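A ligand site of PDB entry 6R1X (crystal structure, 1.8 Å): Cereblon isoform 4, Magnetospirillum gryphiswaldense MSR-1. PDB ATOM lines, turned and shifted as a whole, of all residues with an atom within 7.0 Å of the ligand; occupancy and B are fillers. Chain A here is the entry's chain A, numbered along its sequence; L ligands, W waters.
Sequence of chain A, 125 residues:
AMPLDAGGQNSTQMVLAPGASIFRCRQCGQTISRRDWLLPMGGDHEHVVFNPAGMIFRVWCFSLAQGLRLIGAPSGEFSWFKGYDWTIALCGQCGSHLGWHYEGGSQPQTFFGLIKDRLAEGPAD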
ATOM      1  N   VAL A  49       4.231 -18.363   9.728  1.00  0.00           N
ATOM      2  CA  VAL A  49       3.819 -17.317   8.806  1.00  0.00           C
ATOM      3  C   VAL A  49       4.840 -17.166   7.691  1.00  0.00           C
ATOM      4  O   VAL A  49       5.982 -17.584   7.822  1.00  0.00           O
ATOM      5  CB  VAL A  49       3.632 -15.971   9.550  1.00  0.00           C
ATOM      6  CG1 VAL A  49       2.416 -16.048  10.479  1.00  0.00           C
ATOM      7  CG2 VAL A  49       4.870 -15.581  10.333  1.00  0.00           C
ATOM      8  N   PHE A  50       4.415 -16.541   6.592  1.00  0.00           N
ATOM      9  CA  PHE A  50       5.309 -16.258   5.499  1.00  0.00           C
ATOM     10  C   PHE A  50       5.217 -14.765   5.148  1.00  0.00           C
ATOM     11  O   PHE A  50       4.152 -14.147   5.240  1.00  0.00           O
ATOM     12  CB  PHE A  50       4.932 -17.047   4.241  1.00  0.00           C
ATOM     13  CG  PHE A  50       5.101 -18.532   4.312  1.00  0.00           C
ATOM     14  CD1 PHE A  50       4.066 -19.361   4.772  1.00  0.00           C
ATOM     15  CD2 PHE A  50       6.213 -19.139   3.759  1.00  0.00           C
ATOM     16  CE1 PHE A  50       4.234 -20.740   4.771  1.00  0.00           C
ATOM     17  CE2 PHE A  50       6.381 -20.518   3.772  1.00  0.00           C
ATOM     18  CZ  PHE A  50       5.383 -21.325   4.264  1.00  0.00           C
ATOM     19  N   ASN A  51       6.344 -14.193   4.756  1.00  0.00           N
ATOM     20  CA  ASN A  51       6.384 -12.817   4.275  1.00  0.00           C
ATOM     21  C   ASN A  51       6.244 -12.765   2.725  1.00  0.00           C
ATOM     22  O   ASN A  51       6.164 -13.819   2.079  1.00  0.00           O
ATOM     23  CB  ASN A  51       7.616 -12.080   4.848  1.00  0.00           C
ATOM     24  CG  ASN A  51       8.930 -12.510   4.230  1.00  0.00           C
ATOM     25  OD1 ASN A  51       8.986 -13.260   3.234  1.00  0.00           O
ATOM     26  ND2 ASN A  51      10.031 -12.008   4.800  1.00  0.00           N
ATOM     27  N   PRO A  52       6.211 -11.560   2.123  1.00  0.00           N
ATOM     28  CA  PRO A  52       6.030 -11.506   0.664  1.00  0.00           C
ATOM     29  C   PRO A  52       7.194 -12.069  -0.164  1.00  0.00           C
ATOM     30  O   PRO A  52       7.012 -12.393  -1.336  1.00  0.00           O
ATOM     31  CB  PRO A  52       5.819  -9.996   0.378  1.00  0.00           C
ATOM     32  CG  PRO A  52       5.327  -9.438   1.688  1.00  0.00           C
ATOM     33  CD  PRO A  52       6.054 -10.222   2.748  1.00  0.00           C
ATOM     34  N   ALA A  53       8.363 -12.184   0.457  1.00  0.00           N
ATOM     35  CA  ALA A  53       9.523 -12.825  -0.139  1.00  0.00           C
ATOM     36  C   ALA A  53       9.515 -14.346   0.009  1.00  0.00           C
ATOM     37  O   ALA A  53      10.486 -15.016  -0.345  1.00  0.00           O
ATOM     38  CB  ALA A  53      10.781 -12.259   0.493  1.00  0.00           C
ATOM     39  N   MET A  55       9.573 -16.172   2.708  1.00  0.00           N
ATOM     40  CA  MET A  55      10.319 -16.710   3.844  1.00  0.00           C
ATOM     41  C   MET A  55       9.306 -17.144   4.893  1.00  0.00           C
ATOM     42  O   MET A  55       8.406 -16.377   5.243  1.00  0.00           O
ATOM     43  CB  MET A  55      11.208 -15.642   4.477  1.00  0.00           C
ATOM     44  CG  MET A  55      12.244 -15.027   3.605  1.00  0.00           C
ATOM     45  SD  MET A  55      13.736 -14.830   4.647  1.00  0.00           S
ATOM     46  CE  MET A  55      13.764 -16.305   5.663  1.00  0.00           C
ATOM     47  N   PHE A  57       8.540 -18.198   8.754  1.00  0.00           N
ATOM     48  CA  PHE A  57       9.058 -17.942  10.095  1.00  0.00           C
ATOM     49  C   PHE A  57       8.135 -18.641  11.062  1.00  0.00           C
ATOM     50  O   PHE A  57       6.896 -18.581  10.953  1.00  0.00           O
ATOM     51  CB  PHE A  57       9.038 -16.463  10.412  1.00  0.00           C
ATOM     52  CG  PHE A  57       9.850 -15.618   9.480  1.00  0.00           C
ATOM     53  CD1 PHE A  57      11.213 -15.419   9.703  1.00  0.00           C
ATOM     54  CD2 PHE A  57       9.256 -14.984   8.424  1.00  0.00           C
ATOM     55  CE1 PHE A  57      11.970 -14.628   8.861  1.00  0.00           C
ATOM     56  CE2 PHE A  57      10.018 -14.186   7.567  1.00  0.00           C
ATOM     57  CZ  PHE A  57      11.354 -13.959   7.823  1.00  0.00           C
ATOM     58  N   SER A  75       5.216  -0.109  10.231  1.00  0.00           N
ATOM     59  CA  SER A  75       4.466  -0.334   9.012  1.00  0.00           C
ATOM     60  C   SER A  75       3.349  -1.334   9.231  1.00  0.00           C
ATOM     61  O   SER A  75       3.537  -2.352   9.888  1.00  0.00           O
ATOM     62  CB  SER A  75       5.399  -0.864   7.900  1.00  0.00           C
ATOM     63  OG  SER A  75       4.621  -1.062   6.715  1.00  0.00           O
ATOM     64  N   GLY A  76       2.178  -1.105   8.658  1.00  0.00           N
ATOM     65  CA  GLY A  76       1.067  -2.079   8.714  1.00  0.00           C
ATOM     66  C   GLY A  76       1.117  -3.052   7.536  1.00  0.00           C
ATOM     67  O   GLY A  76       0.342  -4.014   7.500  1.00  0.00           O
ATOM     68  N   GLU A  77       2.004  -2.823   6.583  1.00  0.00           N
ATOM     69  CA  GLU A  77       2.029  -3.588   5.313  1.00  0.00           C
ATOM     70  C   GLU A  77       2.282  -5.070   5.581  1.00  0.00           C
ATOM     71  O   GLU A  77       3.251  -5.406   6.244  1.00  0.00           O
ATOM     72  CB  GLU A  77       3.076  -3.058   4.343  1.00  0.00           C
ATOM     73  CG  GLU A  77       2.792  -1.611   3.913  1.00  0.00           C
ATOM     74  CD  GLU A  77       3.731  -1.055   2.857  1.00  0.00           C
ATOM     75  OE1 GLU A  77       4.811  -1.641   2.630  1.00  0.00           O
ATOM     76  OE2 GLU A  77       3.362  -0.002   2.259  1.00  0.00           O
ATOM     77  N   PHE A  78       1.379  -5.913   5.118  1.00  0.00           N
ATOM     78  CA  PHE A  78       1.447  -7.354   5.276  1.00  0.00           C
ATOM     79  C   PHE A  78       1.548  -7.837   6.728  1.00  0.00           C
ATOM     80  O   PHE A  78       2.043  -8.919   6.967  1.00  0.00           O
ATOM     81  CB  PHE A  78       2.668  -7.913   4.476  1.00  0.00           C
ATOM     82  CG  PHE A  78       2.720  -7.419   3.062  1.00  0.00           C
ATOM     83  CD1 PHE A  78       1.800  -7.879   2.123  1.00  0.00           C
ATOM     84  CD2 PHE A  78       3.664  -6.473   2.691  1.00  0.00           C
ATOM     85  CE1 PHE A  78       1.853  -7.433   0.813  1.00  0.00           C
ATOM     86  CE2 PHE A  78       3.718  -6.015   1.375  1.00  0.00           C
ATOM     87  CZ  PHE A  78       2.817  -6.507   0.438  1.00  0.00           C
ATOM     88  N   SER A  79       1.037  -7.078   7.687  1.00  0.00           N
ATOM     89  CA  SER A  79       1.123  -7.471   9.068  1.00  0.00           C
ATOM     90  C   SER A  79       0.384  -8.777   9.296  1.00  0.00           C
ATOM     91  O   SER A  79      -0.730  -8.961   8.858  1.00  0.00           O
ATOM     92  CB  SER A  79       0.561  -6.421  10.028  1.00  0.00           C
ATOM     93  OG  SER A  79       0.737  -6.885  11.358  1.00  0.00           O
ATOM     94  N   TRP A  80       1.043  -9.683   9.995  1.00  0.00           N
ATOM     95  CA  TRP A  80       0.488 -10.976  10.314  1.00  0.00           C
ATOM     96  C   TRP A  80      -0.483 -10.897  11.493  1.00  0.00           C
ATOM     97  O   TRP A  80      -1.165 -11.884  11.788  1.00  0.00           O
ATOM     98  CB  TRP A  80       1.599 -11.948  10.712  1.00  0.00           C
ATOM     99  CG  TRP A  80       2.543 -12.257   9.610  1.00  0.00           C
ATOM    100  CD1 TRP A  80       2.226 -12.625   8.338  1.00  0.00           C
ATOM    101  CD2 TRP A  80       3.959 -12.290   9.699  1.00  0.00           C
ATOM    102  NE1 TRP A  80       3.355 -12.837   7.611  1.00  0.00           N
ATOM    103  CE2 TRP A  80       4.440 -12.659   8.430  1.00  0.00           C
ATOM    104  CE3 TRP A  80       4.864 -12.029  10.716  1.00  0.00           C
ATOM    105  CZ2 TRP A  80       5.797 -12.794   8.164  1.00  0.00           C
ATOM    106  CZ3 TRP A  80       6.207 -12.180  10.451  1.00  0.00           C
ATOM    107  CH2 TRP A  80       6.661 -12.524   9.179  1.00  0.00           C
ATOM    108  N   PHE A  81      -0.543  -9.752  12.189  1.00  0.00           N
ATOM    109  CA  PHE A  81      -1.380  -9.634  13.368  1.00  0.00           C
ATOM    110  C   PHE A  81      -2.296  -8.448  13.172  1.00  0.00           C
ATOM    111  O   PHE A  81      -1.844  -7.292  13.050  1.00  0.00           O
ATOM    112  CB  PHE A  81      -0.527  -9.515  14.625  1.00  0.00           C
ATOM    113  CG  PHE A  81       0.398 -10.694  14.835  1.00  0.00           C
ATOM    114  CD1 PHE A  81      -0.046 -11.809  15.521  1.00  0.00           C
ATOM    115  CD2 PHE A  81       1.695 -10.662  14.393  1.00  0.00           C
ATOM    116  CE1 PHE A  81       0.795 -12.883  15.754  1.00  0.00           C
ATOM    117  CE2 PHE A  81       2.559 -11.759  14.600  1.00  0.00           C
ATOM    118  CZ  PHE A  81       2.105 -12.865  15.288  1.00  0.00           C
ATOM    119  N   TYR A  84      -2.014  -4.458  14.163  1.00  0.00           N
ATOM    120  CA  TYR A  84      -0.655  -4.066  14.567  1.00  0.00           C
ATOM    121  C   TYR A  84       0.238  -3.704  13.429  1.00  0.00           C
ATOM    122  O   TYR A  84       0.166  -4.314  12.350  1.00  0.00           O
ATOM    123  CB  TYR A  84       0.036  -5.173  15.344  1.00  0.00           C
ATOM    124  CG  TYR A  84      -0.645  -5.548  16.592  1.00  0.00           C
ATOM    125  CD1 TYR A  84      -1.591  -6.554  16.589  1.00  0.00           C
ATOM    126  CD2 TYR A  84      -0.318  -4.948  17.789  1.00  0.00           C
ATOM    127  CE1 TYR A  84      -2.209  -6.964  17.763  1.00  0.00           C
ATOM    128  CE2 TYR A  84      -0.951  -5.318  18.945  1.00  0.00           C
ATOM    129  CZ  TYR A  84      -1.896  -6.340  18.928  1.00  0.00           C
ATOM    130  OH  TYR A  84      -2.502  -6.734  20.086  1.00  0.00           O
ATOM    131  N   ASP A  85       1.058  -2.690  13.676  1.00  0.00           N
ATOM    132  CA  ASP A  85       2.093  -2.239  12.781  1.00  0.00           C
ATOM    133  C   ASP A  85       3.380  -2.821  13.335  1.00  0.00           C
ATOM    134  O   ASP A  85       3.543  -2.966  14.556  1.00  0.00           O
ATOM    135  CB  ASP A  85       2.136  -0.728  12.771  1.00  0.00           C
ATOM    136  CG  ASP A  85       0.786  -0.133  12.404  1.00  0.00           C
ATOM    137  OD1 ASP A  85       0.252  -0.585  11.404  1.00  0.00           O
ATOM    138  OD2 ASP A  85       0.232   0.696  13.187  1.00  0.00           O
ATOM    139  N   TRP A  86       4.319  -3.125  12.455  1.00  0.00           N
ATOM    140  CA  TRP A  86       5.556  -3.748  12.892  1.00  0.00           C
ATOM    141  C   TRP A  86       6.751  -2.921  12.583  1.00  0.00           C
ATOM    142  O   TRP A  86       6.760  -2.100  11.648  1.00  0.00           O
ATOM    143  CB  TRP A  86       5.712  -5.140  12.270  1.00  0.00           C
ATOM    144  CG  TRP A  86       5.525  -5.207  10.749  1.00  0.00           C
ATOM    145  CD1 TRP A  86       4.352  -5.473  10.072  1.00  0.00           C
ATOM    146  CD2 TRP A  86       6.515  -4.953   9.750  1.00  0.00           C
ATOM    147  NE1 TRP A  86       4.585  -5.455   8.718  1.00  0.00           N
ATOM    148  CE2 TRP A  86       5.891  -5.119   8.490  1.00  0.00           C
ATOM    149  CE3 TRP A  86       7.859  -4.595   9.798  1.00  0.00           C
ATOM    150  CZ2 TRP A  86       6.583  -4.957   7.280  1.00  0.00           C
ATOM    151  CZ3 TRP A  86       8.550  -4.446   8.594  1.00  0.00           C
ATOM    152  CH2 TRP A  86       7.896  -4.625   7.338  1.00  0.00           C
ATOM    153  N   THR A  87       7.779  -3.139  13.402  1.00  0.00           N
ATOM    154  CA  THR A  87       9.103  -2.603  13.162  1.00  0.00           C
ATOM    155  C   THR A  87      10.047  -3.794  13.261  1.00  0.00           C
ATOM    156  O   THR A  87       9.848  -4.663  14.095  1.00  0.00           O
ATOM    157  CB  THR A  87       9.509  -1.516  14.169  1.00  0.00           C
ATOM    158  OG1 THR A  87       9.675  -2.081  15.474  1.00  0.00           O
ATOM    159  CG2 THR A  87       8.479  -0.374  14.227  1.00  0.00           C
ATOM    160  N   ILE A  88      11.048  -3.814  12.396  1.00  0.00           N
ATOM    161  CA  ILE A  88      12.062  -4.867  12.444  1.00  0.00           C
ATOM    162  C   ILE A  88      12.861  -4.764  13.758  1.00  0.00           C
ATOM    163  O   ILE A  88      13.277  -3.677  14.200  1.00  0.00           O
ATOM    164  CB  ILE A  88      12.978  -4.735  11.220  1.00  0.00           C
ATOM    165  CG1 ILE A  88      12.214  -5.288   9.999  1.00  0.00           C
ATOM    166  CG2 ILE A  88      14.277  -5.498  11.413  1.00  0.00           C
ATOM    167  CD1 ILE A  88      12.841  -4.977   8.670  1.00  0.00           C
ATOM    168  N   HIS A  97      18.723 -10.453  12.510  1.00  0.00           N
ATOM    169  CA  HIS A  97      17.313 -10.202  12.518  1.00  0.00           C
ATOM    170  C   HIS A  97      16.595 -11.202  13.422  1.00  0.00           C
ATOM    171  O   HIS A  97      16.499 -12.385  13.093  1.00  0.00           O
ATOM    172  CB  HIS A  97      16.776 -10.254  11.089  1.00  0.00           C
ATOM    173  CG  HIS A  97      15.310 -10.038  11.023  1.00  0.00           C
ATOM    174  ND1 HIS A  97      14.497 -10.716  10.137  1.00  0.00           N
ATOM    175  CD2 HIS A  97      14.493  -9.267  11.785  1.00  0.00           C
ATOM    176  CE1 HIS A  97      13.252 -10.346  10.345  1.00  0.00           C
ATOM    177  NE2 HIS A  97      13.223  -9.446  11.309  1.00  0.00           N
ATOM    178  N   TRP A 100      10.284  -8.959  15.197  1.00  0.00           N
ATOM    179  CA  TRP A 100       9.580  -7.695  15.022  1.00  0.00           C
ATOM    180  C   TRP A 100       9.019  -7.236  16.349  1.00  0.00           C
ATOM    181  O   TRP A 100       8.658  -8.038  17.185  1.00  0.00           O
ATOM    182  CB  TRP A 100       8.399  -7.863  14.044  1.00  0.00           C
ATOM    183  CG  TRP A 100       8.828  -8.337  12.704  1.00  0.00           C
ATOM    184  CD1 TRP A 100       9.158  -7.547  11.643  1.00  0.00           C
ATOM    185  CD2 TRP A 100       9.061  -9.677  12.312  1.00  0.00           C
ATOM    186  NE1 TRP A 100       9.518  -8.335  10.594  1.00  0.00           N
ATOM    187  CE2 TRP A 100       9.492  -9.649  10.984  1.00  0.00           C
ATOM    188  CE3 TRP A 100       8.946 -10.921  12.944  1.00  0.00           C
ATOM    189  CZ2 TRP A 100       9.822 -10.797  10.283  1.00  0.00           C
ATOM    190  CZ3 TRP A 100       9.310 -12.074  12.239  1.00  0.00           C
ATOM    191  CH2 TRP A 100       9.743 -11.993  10.921  1.00  0.00           C
ATOM    192  N   TYR A 102       5.678  -5.203  17.572  1.00  0.00           N
ATOM    193  CA  TYR A 102       4.346  -4.849  17.082  1.00  0.00           C
ATOM    194  C   TYR A 102       3.790  -3.768  17.964  1.00  0.00           C
ATOM    195  O   TYR A 102       3.968  -3.820  19.167  1.00  0.00           O
ATOM    196  CB  TYR A 102       3.458  -6.073  17.069  1.00  0.00           C
ATOM    197  CG  TYR A 102       3.860  -7.013  15.949  1.00  0.00           C
ATOM    198  CD1 TYR A 102       3.363  -6.849  14.663  1.00  0.00           C
ATOM    199  CD2 TYR A 102       4.757  -8.044  16.163  1.00  0.00           C
ATOM    200  CE1 TYR A 102       3.693  -7.704  13.622  1.00  0.00           C
ATOM    201  CE2 TYR A 102       5.112  -8.907  15.139  1.00  0.00           C
ATOM    202  CZ  TYR A 102       4.621  -8.708  13.861  1.00  0.00           C
ATOM    203  OH  TYR A 102       5.004  -9.558  12.820  1.00  0.00           O
HETATM  204  C1  LIG L   1       6.893  -9.227   8.249  1.00  0.00           C
HETATM  205  C2  LIG L   1       8.983  -8.934   7.089  1.00  0.00           C
HETATM  206  C3  LIG L   1      10.021  -7.969   6.657  1.00  0.00           C
HETATM  207  C4  LIG L   1      11.320  -8.255   6.419  1.00  0.00           C
HETATM  208  C5  LIG L   1      12.248  -7.240   5.811  1.00  0.00           C
HETATM  209  C6  LIG L   1      11.982  -9.567   6.725  1.00  0.00           C
HETATM  210  N1  LIG L   1       4.569  -9.257   8.146  1.00  0.00           N
HETATM  211  N2  LIG L   1       7.901  -8.393   7.671  1.00  0.00           N
HETATM  212  C7  LIG L   1       6.329  -8.697   9.573  1.00  0.00           C
HETATM  213  O1  LIG L   1       5.688  -9.453   6.137  1.00  0.00           O
HETATM  214  C8  LIG L   1       5.673  -9.326   7.351  1.00  0.00           C
HETATM  215  C9  LIG L   1       4.845  -8.930   9.456  1.00  0.00           C
HETATM  216  O2  LIG L   1       4.029  -8.969  10.353  1.00  0.00           O
HETATM  217  O3  LIG L   1       9.103 -10.143   6.917  1.00  0.00           O
HETATM  218  O   HOH W   1       7.189  -7.106   4.081  1.00  0.00           O
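O2 of the ligand sits at hydrogen-bond distance from OH of Tyr 102, 2.7 Å away.
O of Phe 78 lies within hydrogen-bond range of N1 of the ligand, at 2.8 Å.
An oxygen (O3) of the ligand is in hydrogen-bond range of the side-chain amide nitrogen of Asn 51 (3.0 Å).
The backbone NH of Trp 80 lies within hydrogen-bond range of an oxygen (O2) of the ligand, at 3.1 Å.
The backbone NH (N) of Met 55 is in hydrogen-bond range of the side-chain amide oxygen (OD1) of Asn 51 (3.0 Å).
The side-chain amide oxygen of Asn 51 lies within hydrogen-bond range of the backbone NH of Ala 53 (3.0 Å).
The indole nitrogen (NE1) of Trp 80 is in hydrogen-bond range of the backbone carbonyl oxygen (O) of Phe 50, 2.8 Å away.
The side-chain hydroxyl (OG) of Ser 79 is in hydrogen-bond range of the backbone carbonyl oxygen (O) of Phe 81 (3.1 Å).
O of Tyr 84 sits at hydrogen-bond distance from OG of Ser 79 (2.8 Å).
NE1 of Trp 86 sits at hydrogen-bond distance from O of Glu 77 (2.8 Å).
O of Ser 75 is in hydrogen-bond range of N of Trp 86, 2.8 Å away.
The indole nitrogen (NE1) of Trp 100 lies close to a nitrogen (N2) of the ligand.
Merely in contact with the ligand: Pro 52 (3.5 Å), Ser 79 (3.5 Å), Trp 86 (3.5 Å), Ile 88 (3.7 Å) and His 97 (3.9 Å).
Hydrophobic or aromatic side chains that line the ligand: Pro 52, Phe 78, Trp 80, Trp 86, Ile 88, His 97, Trp 100 and Tyr 102.
Within 4 Å of the ligand: Asn 51, Pro 52, Phe 78, Ser 79, Trp 80, Trp 86, Ile 88, His 97, Trp 100 and Tyr 102.
The nearest printed residue that does not touch the ligand is Phe 57 (4.2 Å).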
